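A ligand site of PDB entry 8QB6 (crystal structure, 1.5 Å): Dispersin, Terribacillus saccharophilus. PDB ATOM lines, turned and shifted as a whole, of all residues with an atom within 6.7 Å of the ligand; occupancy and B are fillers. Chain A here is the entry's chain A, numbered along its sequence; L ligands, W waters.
O3 of the ligand lies within hydrogen-bond range of OE2 of Glu 300. A nitrogen (N1) of the ligand sits at hydrogen-bond distance from the side-chain carboxylate of Asp 160 (3.0 Å). O1 of the ligand is in hydrogen-bond range of OH of Tyr 247 (2.7 Å). The guanidinium group (NH1) of Arg 13 lies within hydrogen-bond range of an oxygen (O3) of the ligand (2.8 Å).
The guanidinium group (NH2) of Arg 13 is in salt-bridge range of the side-chain carboxylate (OD1) of Asp 42, 3.3 Å away. The guanidinium group (NH1) of Arg 13 lies within salt-bridge range of the side-chain carboxylate (OD2) of Asp 10, at 2.9 Å. A ring nitrogen (NE2) of His 93 lies within hydrogen-bond range of the side-chain carboxylate (OE1) of Glu 161, at 2.7 Å. OD2 of Asp 160 lies within hydrogen-bond range of NE2 of His 93, 3.3 Å away. The side-chain carboxylate of Asp 42 lies within hydrogen-bond range of a ring nitrogen (ND1) of His 93, 2.6 Å away. The side-chain carboxylate (OE1) of Glu 300 is in salt-bridge range of the guanidinium group (NH1) of Arg 13 (3.9 Å). The side-chain carboxylate (OD2) of Asp 195 sits at hydrogen-bond distance from the backbone NH (N) of Glu 161 (2.7 Å). NE1 of Trp 214 sits at hydrogen-bond distance from OD1 of Asp 195 (2.9 Å).
His 93 touches the ligand (CE1 to O2, 3.3 Å). Glu 161 touches the ligand. Trp 193 touches the ligand. Trp 214 touches the ligand. Trp 298 touches the ligand. Of the 21 residues printed, 9 come within 4 Å of the ligand.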
ATOM      1  N   ASP A  10      26.289  26.289   7.055  1.00  0.00           N
ATOM      2  CA  ASP A  10      26.681  25.069   6.352  1.00  0.00           C
ATOM      3  C   ASP A  10      27.315  25.472   5.013  1.00  0.00           C
ATOM      4  O   ASP A  10      26.597  25.701   4.032  1.00  0.00           O
ATOM      5  CB  ASP A  10      25.492  24.148   6.110  1.00  0.00           C
ATOM      6  CG  ASP A  10      25.753  22.931   5.254  1.00  0.00           C
ATOM      7  OD1 ASP A  10      26.938  22.666   4.952  1.00  0.00           O
ATOM      8  OD2 ASP A  10      24.739  22.256   4.910  1.00  0.00           O
ATOM      9  N   ARG A  13      27.513  21.946   2.094  1.00  0.00           N
ATOM     10  CA  ARG A  13      26.491  21.572   1.108  1.00  0.00           C
ATOM     11  C   ARG A  13      26.385  22.643   0.024  1.00  0.00           C
ATOM     12  O   ARG A  13      25.859  22.378  -1.059  1.00  0.00           O
ATOM     13  CB  ARG A  13      25.123  21.349   1.783  1.00  0.00           C
ATOM     14  CG  ARG A  13      24.906  19.969   2.398  1.00  0.00           C
ATOM     15  CD  ARG A  13      25.980  19.573   3.422  1.00  0.00           C
ATOM     16  NE  ARG A  13      25.582  18.391   4.181  1.00  0.00           N
ATOM     17  CZ  ARG A  13      24.656  18.373   5.156  1.00  0.00           C
ATOM     18  NH1 ARG A  13      24.234  19.510   5.704  1.00  0.00           N
ATOM     19  NH2 ARG A  13      24.094  17.241   5.548  1.00  0.00           N
ATOM     20  N   HIS A  39      30.180  25.246   9.628  1.00  0.00           N
ATOM     21  CA  HIS A  39      30.004  23.836   9.351  1.00  0.00           C
ATOM     22  C   HIS A  39      30.582  23.568   7.960  1.00  0.00           C
ATOM     23  O   HIS A  39      29.913  23.608   6.928  1.00  0.00           O
ATOM     24  CB  HIS A  39      28.522  23.473   9.480  1.00  0.00           C
ATOM     25  CG  HIS A  39      28.164  22.055   9.235  1.00  0.00           C
ATOM     26  ND1 HIS A  39      27.934  21.209  10.320  1.00  0.00           N
ATOM     27  CD2 HIS A  39      27.902  21.343   8.093  1.00  0.00           C
ATOM     28  CE1 HIS A  39      27.622  19.989   9.815  1.00  0.00           C
ATOM     29  NE2 HIS A  39      27.582  20.063   8.471  1.00  0.00           N
ATOM     30  N   ASP A  42      31.146  17.849   5.719  1.00  0.00           N
ATOM     31  CA  ASP A  42      29.982  16.982   5.667  1.00  0.00           C
ATOM     32  C   ASP A  42      30.196  15.987   4.544  1.00  0.00           C
ATOM     33  O   ASP A  42      31.304  15.836   4.057  1.00  0.00           O
ATOM     34  CB  ASP A  42      28.685  17.808   5.577  1.00  0.00           C
ATOM     35  CG  ASP A  42      27.560  17.131   6.331  1.00  0.00           C
ATOM     36  OD1 ASP A  42      27.175  16.008   5.889  1.00  0.00           O
ATOM     37  OD2 ASP A  42      27.059  17.713   7.341  1.00  0.00           O
ATOM     38  N   ASP A  89      32.370  17.457  11.394  1.00  0.00           N
ATOM     39  CA  ASP A  89      31.395  16.487  11.816  1.00  0.00           C
ATOM     40  C   ASP A  89      32.000  15.092  11.868  1.00  0.00           C
ATOM     41  O   ASP A  89      32.503  14.595  10.850  1.00  0.00           O
ATOM     42  CB  ASP A  89      30.184  16.488  10.897  1.00  0.00           C
ATOM     43  CG  ASP A  89      28.969  15.919  11.593  1.00  0.00           C
ATOM     44  OD1 ASP A  89      29.132  14.876  12.241  1.00  0.00           O
ATOM     45  OD2 ASP A  89      27.874  16.518  11.422  1.00  0.00           O
ATOM     46  N   HIS A  93      28.650  11.829   8.669  1.00  0.00           N
ATOM     47  CA  HIS A  93      28.705  13.096   7.936  1.00  0.00           C
ATOM     48  C   HIS A  93      30.159  13.409   7.555  1.00  0.00           C
ATOM     49  O   HIS A  93      30.597  14.576   7.493  1.00  0.00           O
ATOM     50  CB  HIS A  93      28.115  14.233   8.781  1.00  0.00           C
ATOM     51  CG  HIS A  93      26.625  14.187   8.779  1.00  0.00           C
ATOM     52  ND1 HIS A  93      25.858  14.643   7.734  1.00  0.00           N
ATOM     53  CD2 HIS A  93      25.785  13.735   9.732  1.00  0.00           C
ATOM     54  CE1 HIS A  93      24.566  14.417   8.034  1.00  0.00           C
ATOM     55  NE2 HIS A  93      24.476  13.910   9.240  1.00  0.00           N
ATOM     56  N   ASP A 160      26.151  13.901  15.127  1.00  0.00           N
ATOM     57  CA  ASP A 160      24.770  13.792  14.664  1.00  0.00           C
ATOM     58  C   ASP A 160      24.567  12.595  13.733  1.00  0.00           C
ATOM     59  O   ASP A 160      25.389  12.336  12.827  1.00  0.00           O
ATOM     60  CB  ASP A 160      24.285  15.065  13.984  1.00  0.00           C
ATOM     61  CG  ASP A 160      25.091  15.568  12.809  1.00  0.00           C
ATOM     62  OD1 ASP A 160      26.362  15.599  12.954  1.00  0.00           O
ATOM     63  OD2 ASP A 160      24.467  15.963  11.793  1.00  0.00           O
ATOM     64  N   GLU A 161      23.387  11.957  13.886  1.00  0.00           N
ATOM     65  CA  GLU A 161      22.856  10.961  12.958  1.00  0.00           C
ATOM     66  C   GLU A 161      23.878   9.844  12.681  1.00  0.00           C
ATOM     67  O   GLU A 161      24.188   9.508  11.524  1.00  0.00           O
ATOM     68  CB  GLU A 161      22.415  11.614  11.652  1.00  0.00           C
ATOM     69  CG  GLU A 161      21.370  12.715  11.845  1.00  0.00           C
ATOM     70  CD  GLU A 161      20.962  13.447  10.576  1.00  0.00           C
ATOM     71  OE1 GLU A 161      21.817  13.661   9.680  1.00  0.00           O
ATOM     72  OE2 GLU A 161      19.746  13.806  10.466  1.00  0.00           O
ATOM     73  N   TRP A 193      26.196  17.527  18.766  1.00  0.00           N
ATOM     74  CA  TRP A 193      24.731  17.521  18.707  1.00  0.00           C
ATOM     75  C   TRP A 193      24.195  16.482  19.701  1.00  0.00           C
ATOM     76  O   TRP A 193      24.855  15.570  20.153  1.00  0.00           O
ATOM     77  CB  TRP A 193      24.300  17.201  17.274  1.00  0.00           C
ATOM     78  CG  TRP A 193      24.852  18.150  16.241  1.00  0.00           C
ATOM     79  CD1 TRP A 193      25.956  17.940  15.474  1.00  0.00           C
ATOM     80  CD2 TRP A 193      24.350  19.439  15.865  1.00  0.00           C
ATOM     81  NE1 TRP A 193      26.169  19.006  14.634  1.00  0.00           N
ATOM     82  CE2 TRP A 193      25.182  19.942  14.843  1.00  0.00           C
ATOM     83  CE3 TRP A 193      23.225  20.202  16.231  1.00  0.00           C
ATOM     84  CZ2 TRP A 193      24.971  21.161  14.212  1.00  0.00           C
ATOM     85  CZ3 TRP A 193      23.018  21.428  15.612  1.00  0.00           C
ATOM     86  CH2 TRP A 193      23.857  21.895  14.600  1.00  0.00           C
ATOM     87  N   ASP A 195      21.574  14.254  19.346  1.00  0.00           N
ATOM     88  CA  ASP A 195      20.588  13.255  18.874  1.00  0.00           C
ATOM     89  C   ASP A 195      21.035  11.793  19.012  1.00  0.00           C
ATOM     90  O   ASP A 195      20.189  10.906  18.957  1.00  0.00           O
ATOM     91  CB  ASP A 195      20.181  13.564  17.434  1.00  0.00           C
ATOM     92  CG  ASP A 195      21.386  13.467  16.489  1.00  0.00           C
ATOM     93  OD1 ASP A 195      22.114  14.454  16.415  1.00  0.00           O
ATOM     94  OD2 ASP A 195      21.622  12.367  15.923  1.00  0.00           O
ATOM     95  N   LEU A 212      24.528  20.708  21.458  1.00  0.00           N
ATOM     96  CA  LEU A 212      23.715  21.452  20.533  1.00  0.00           C
ATOM     97  C   LEU A 212      22.419  20.667  20.393  1.00  0.00           C
ATOM     98  O   LEU A 212      22.400  19.617  19.774  1.00  0.00           O
ATOM     99  CB  LEU A 212      24.411  21.634  19.173  1.00  0.00           C
ATOM    100  CG  LEU A 212      25.871  22.081  19.198  1.00  0.00           C
ATOM    101  CD1 LEU A 212      26.363  22.339  17.761  1.00  0.00           C
ATOM    102  CD2 LEU A 212      26.149  23.267  20.101  1.00  0.00           C
ATOM    103  N   TRP A 214      19.041  19.990  18.981  1.00  0.00           N
ATOM    104  CA  TRP A 214      18.294  20.389  17.800  1.00  0.00           C
ATOM    105  C   TRP A 214      16.949  19.654  17.725  1.00  0.00           C
ATOM    106  O   TRP A 214      15.976  20.257  17.278  1.00  0.00           O
ATOM    107  CB  TRP A 214      19.087  20.209  16.499  1.00  0.00           C
ATOM    108  CG  TRP A 214      19.485  18.803  16.133  1.00  0.00           C
ATOM    109  CD1 TRP A 214      20.469  18.028  16.709  1.00  0.00           C
ATOM    110  CD2 TRP A 214      18.934  18.013  15.066  1.00  0.00           C
ATOM    111  NE1 TRP A 214      20.529  16.810  16.103  1.00  0.00           N
ATOM    112  CE2 TRP A 214      19.607  16.771  15.075  1.00  0.00           C
ATOM    113  CE3 TRP A 214      17.939  18.238  14.106  1.00  0.00           C
ATOM    114  CZ2 TRP A 214      19.288  15.749  14.184  1.00  0.00           C
ATOM    115  CZ3 TRP A 214      17.650  17.235  13.193  1.00  0.00           C
ATOM    116  CH2 TRP A 214      18.341  16.018  13.215  1.00  0.00           C
ATOM    117  N   GLN A 215      16.915  18.405  18.183  1.00  0.00           N
ATOM    118  CA  GLN A 215      15.680  17.618  18.083  1.00  0.00           C
ATOM    119  C   GLN A 215      15.752  16.431  19.024  1.00  0.00           C
ATOM    120  O   GLN A 215      16.687  15.650  18.964  1.00  0.00           O
ATOM    121  CB  GLN A 215      15.521  17.131  16.646  1.00  0.00           C
ATOM    122  CG  GLN A 215      14.330  16.200  16.402  1.00  0.00           C
ATOM    123  CD  GLN A 215      14.379  15.771  14.962  1.00  0.00           C
ATOM    124  OE1 GLN A 215      15.057  14.823  14.566  1.00  0.00           O
ATOM    125  NE2 GLN A 215      13.743  16.529  14.114  1.00  0.00           N
ATOM    126  N   ALA A 243      15.171  22.528  15.630  1.00  0.00           N
ATOM    127  CA  ALA A 243      15.142  22.152  14.220  1.00  0.00           C
ATOM    128  C   ALA A 243      14.024  22.819  13.428  1.00  0.00           C
ATOM    129  O   ALA A 243      14.082  22.787  12.215  1.00  0.00           O
ATOM    130  CB  ALA A 243      15.010  20.677  14.042  1.00  0.00           C
ATOM    131  N   TYR A 247      16.124  26.459  12.241  1.00  0.00           N
ATOM    132  CA  TYR A 247      16.705  25.971  11.021  1.00  0.00           C
ATOM    133  C   TYR A 247      16.081  26.671   9.827  1.00  0.00           C
ATOM    134  O   TYR A 247      14.870  26.947   9.799  1.00  0.00           O
ATOM    135  CB  TYR A 247      16.505  24.470  10.839  1.00  0.00           C
ATOM    136  CG  TYR A 247      17.419  23.536  11.627  1.00  0.00           C
ATOM    137  CD1 TYR A 247      18.347  23.986  12.557  1.00  0.00           C
ATOM    138  CD2 TYR A 247      17.372  22.161  11.387  1.00  0.00           C
ATOM    139  CE1 TYR A 247      19.176  23.115  13.252  1.00  0.00           C
ATOM    140  CE2 TYR A 247      18.180  21.283  12.084  1.00  0.00           C
ATOM    141  CZ  TYR A 247      19.084  21.757  13.026  1.00  0.00           C
ATOM    142  OH  TYR A 247      20.013  20.939  13.621  1.00  0.00           O
ATOM    143  N   LEU A 249      16.644  26.480   5.367  1.00  0.00           N
ATOM    144  CA  LEU A 249      17.330  25.975   4.206  1.00  0.00           C
ATOM    145  C   LEU A 249      17.118  26.897   3.006  1.00  0.00           C
ATOM    146  O   LEU A 249      16.111  26.797   2.273  1.00  0.00           O
ATOM    147  CB  LEU A 249      16.780  24.565   3.937  1.00  0.00           C
ATOM    148  CG  LEU A 249      17.415  23.437   4.745  1.00  0.00           C
ATOM    149  CD1 LEU A 249      17.053  23.470   6.207  1.00  0.00           C
ATOM    150  CD2 LEU A 249      17.028  22.098   4.147  1.00  0.00           C
ATOM    151  N   THR A 296      20.574  28.309  12.235  1.00  0.00           N
ATOM    152  CA  THR A 296      21.418  27.531  11.316  1.00  0.00           C
ATOM    153  C   THR A 296      20.837  27.589   9.901  1.00  0.00           C
ATOM    154  O   THR A 296      19.665  27.243   9.659  1.00  0.00           O
ATOM    155  CB  THR A 296      21.571  26.066  11.752  1.00  0.00           C
ATOM    156  OG1 THR A 296      22.098  26.024  13.065  1.00  0.00           O
ATOM    157  CG2 THR A 296      22.436  25.306  10.781  1.00  0.00           C
ATOM    158  N   TRP A 298      21.308  25.554   6.694  1.00  0.00           N
ATOM    159  CA  TRP A 298      21.743  24.332   6.046  1.00  0.00           C
ATOM    160  C   TRP A 298      21.668  24.548   4.537  1.00  0.00           C
ATOM    161  O   TRP A 298      20.730  25.202   4.024  1.00  0.00           O
ATOM    162  CB  TRP A 298      20.872  23.143   6.492  1.00  0.00           C
ATOM    163  CG  TRP A 298      20.962  22.828   7.960  1.00  0.00           C
ATOM    164  CD1 TRP A 298      20.005  23.022   8.916  1.00  0.00           C
ATOM    165  CD2 TRP A 298      22.072  22.211   8.641  1.00  0.00           C
ATOM    166  NE1 TRP A 298      20.461  22.639  10.136  1.00  0.00           N
ATOM    167  CE2 TRP A 298      21.718  22.076  10.001  1.00  0.00           C
ATOM    168  CE3 TRP A 298      23.330  21.744   8.226  1.00  0.00           C
ATOM    169  CZ2 TRP A 298      22.583  21.536  10.951  1.00  0.00           C
ATOM    170  CZ3 TRP A 298      24.170  21.204   9.160  1.00  0.00           C
ATOM    171  CH2 TRP A 298      23.797  21.059  10.490  1.00  0.00           C
ATOM    172  N   GLY A 299      22.583  23.882   3.836  1.00  0.00           N
ATOM    173  CA  GLY A 299      22.915  24.202   2.469  1.00  0.00           C
ATOM    174  C   GLY A 299      22.299  23.320   1.367  1.00  0.00           C
ATOM    175  O   GLY A 299      22.443  23.631   0.181  1.00  0.00           O
ATOM    176  N   GLU A 300      21.627  22.238   1.699  1.00  0.00           N
ATOM    177  CA  GLU A 300      21.325  21.229   0.693  1.00  0.00           C
ATOM    178  C   GLU A 300      20.227  21.646  -0.311  1.00  0.00           C
ATOM    179  O   GLU A 300      20.126  20.999  -1.350  1.00  0.00           O
ATOM    180  CB  GLU A 300      21.092  19.847   1.331  1.00  0.00           C
ATOM    181  CG  GLU A 300      19.960  19.757   2.326  1.00  0.00           C
ATOM    182  CD  GLU A 300      20.427  19.921   3.761  1.00  0.00           C
ATOM    183  OE1 GLU A 300      21.037  20.935   4.045  1.00  0.00           O
ATOM    184  OE2 GLU A 300      20.212  19.025   4.554  1.00  0.00           O
ATOM    185  N   HIS A 301      19.458  22.728  -0.039  1.00  0.00           N
ATOM    186  CA  HIS A 301      18.439  23.194  -0.970  1.00  0.00           C
ATOM    187  C   HIS A 301      18.924  24.413  -1.745  1.00  0.00           C
ATOM    188  O   HIS A 301      18.156  25.000  -2.542  1.00  0.00           O
ATOM    189  CB  HIS A 301      17.109  23.477  -0.245  1.00  0.00           C
ATOM    190  CG  HIS A 301      16.479  22.257   0.315  1.00  0.00           C
ATOM    191  ND1 HIS A 301      15.322  22.368   1.065  1.00  0.00           N
ATOM    192  CD2 HIS A 301      16.778  20.950   0.250  1.00  0.00           C
ATOM    193  CE1 HIS A 301      14.937  21.149   1.430  1.00  0.00           C
ATOM    194  NE2 HIS A 301      15.807  20.283   0.946  1.00  0.00           N
HETATM  195  O1  LIG L   1      20.547  18.985  11.830  1.00  0.00           O
HETATM  196  C1  LIG L   1      21.512  18.237  12.048  1.00  0.00           C
HETATM  197  C2  LIG L   1      22.333  18.353  13.296  1.00  0.00           C
HETATM  198  N1  LIG L   1      21.867  17.288  11.174  1.00  0.00           N
HETATM  199  C3  LIG L   1      21.328  17.118   9.836  1.00  0.00           C
HETATM  200  C4  LIG L   1      21.993  18.090   8.862  1.00  0.00           C
HETATM  201  O2  LIG L   1      23.079  17.410   8.230  1.00  0.00           O
HETATM  202  C5  LIG L   1      21.004  18.522   7.778  1.00  0.00           C
HETATM  203  O3  LIG L   1      21.627  19.366   6.808  1.00  0.00           O
HETATM  204  C6  LIG L   1      19.792  17.128   9.732  1.00  0.00           C
HETATM  205  N2  LIG L   1      19.277  18.477   9.565  1.00  0.00           N
HETATM  206  C7  LIG L   1      19.855  19.272   8.442  1.00  0.00           C
HETATM  207  C8  LIG L   1      17.774  18.565   9.455  1.00  0.00           C
HETATM  208  C9  LIG L   1      17.532  19.740   8.553  1.00  0.00           C
HETATM  209  C10 LIG L   1      18.669  19.632   7.545  1.00  0.00           C
HETATM  210  O4  LIG L   1      18.397  18.628   6.576  1.00  0.00           O
HETATM  211  O   HOH W   1      15.660  17.708   5.966  1.00  0.00           O
HETATM  212  O   HOH W   2      25.370  17.576   9.612  1.00  0.00           O
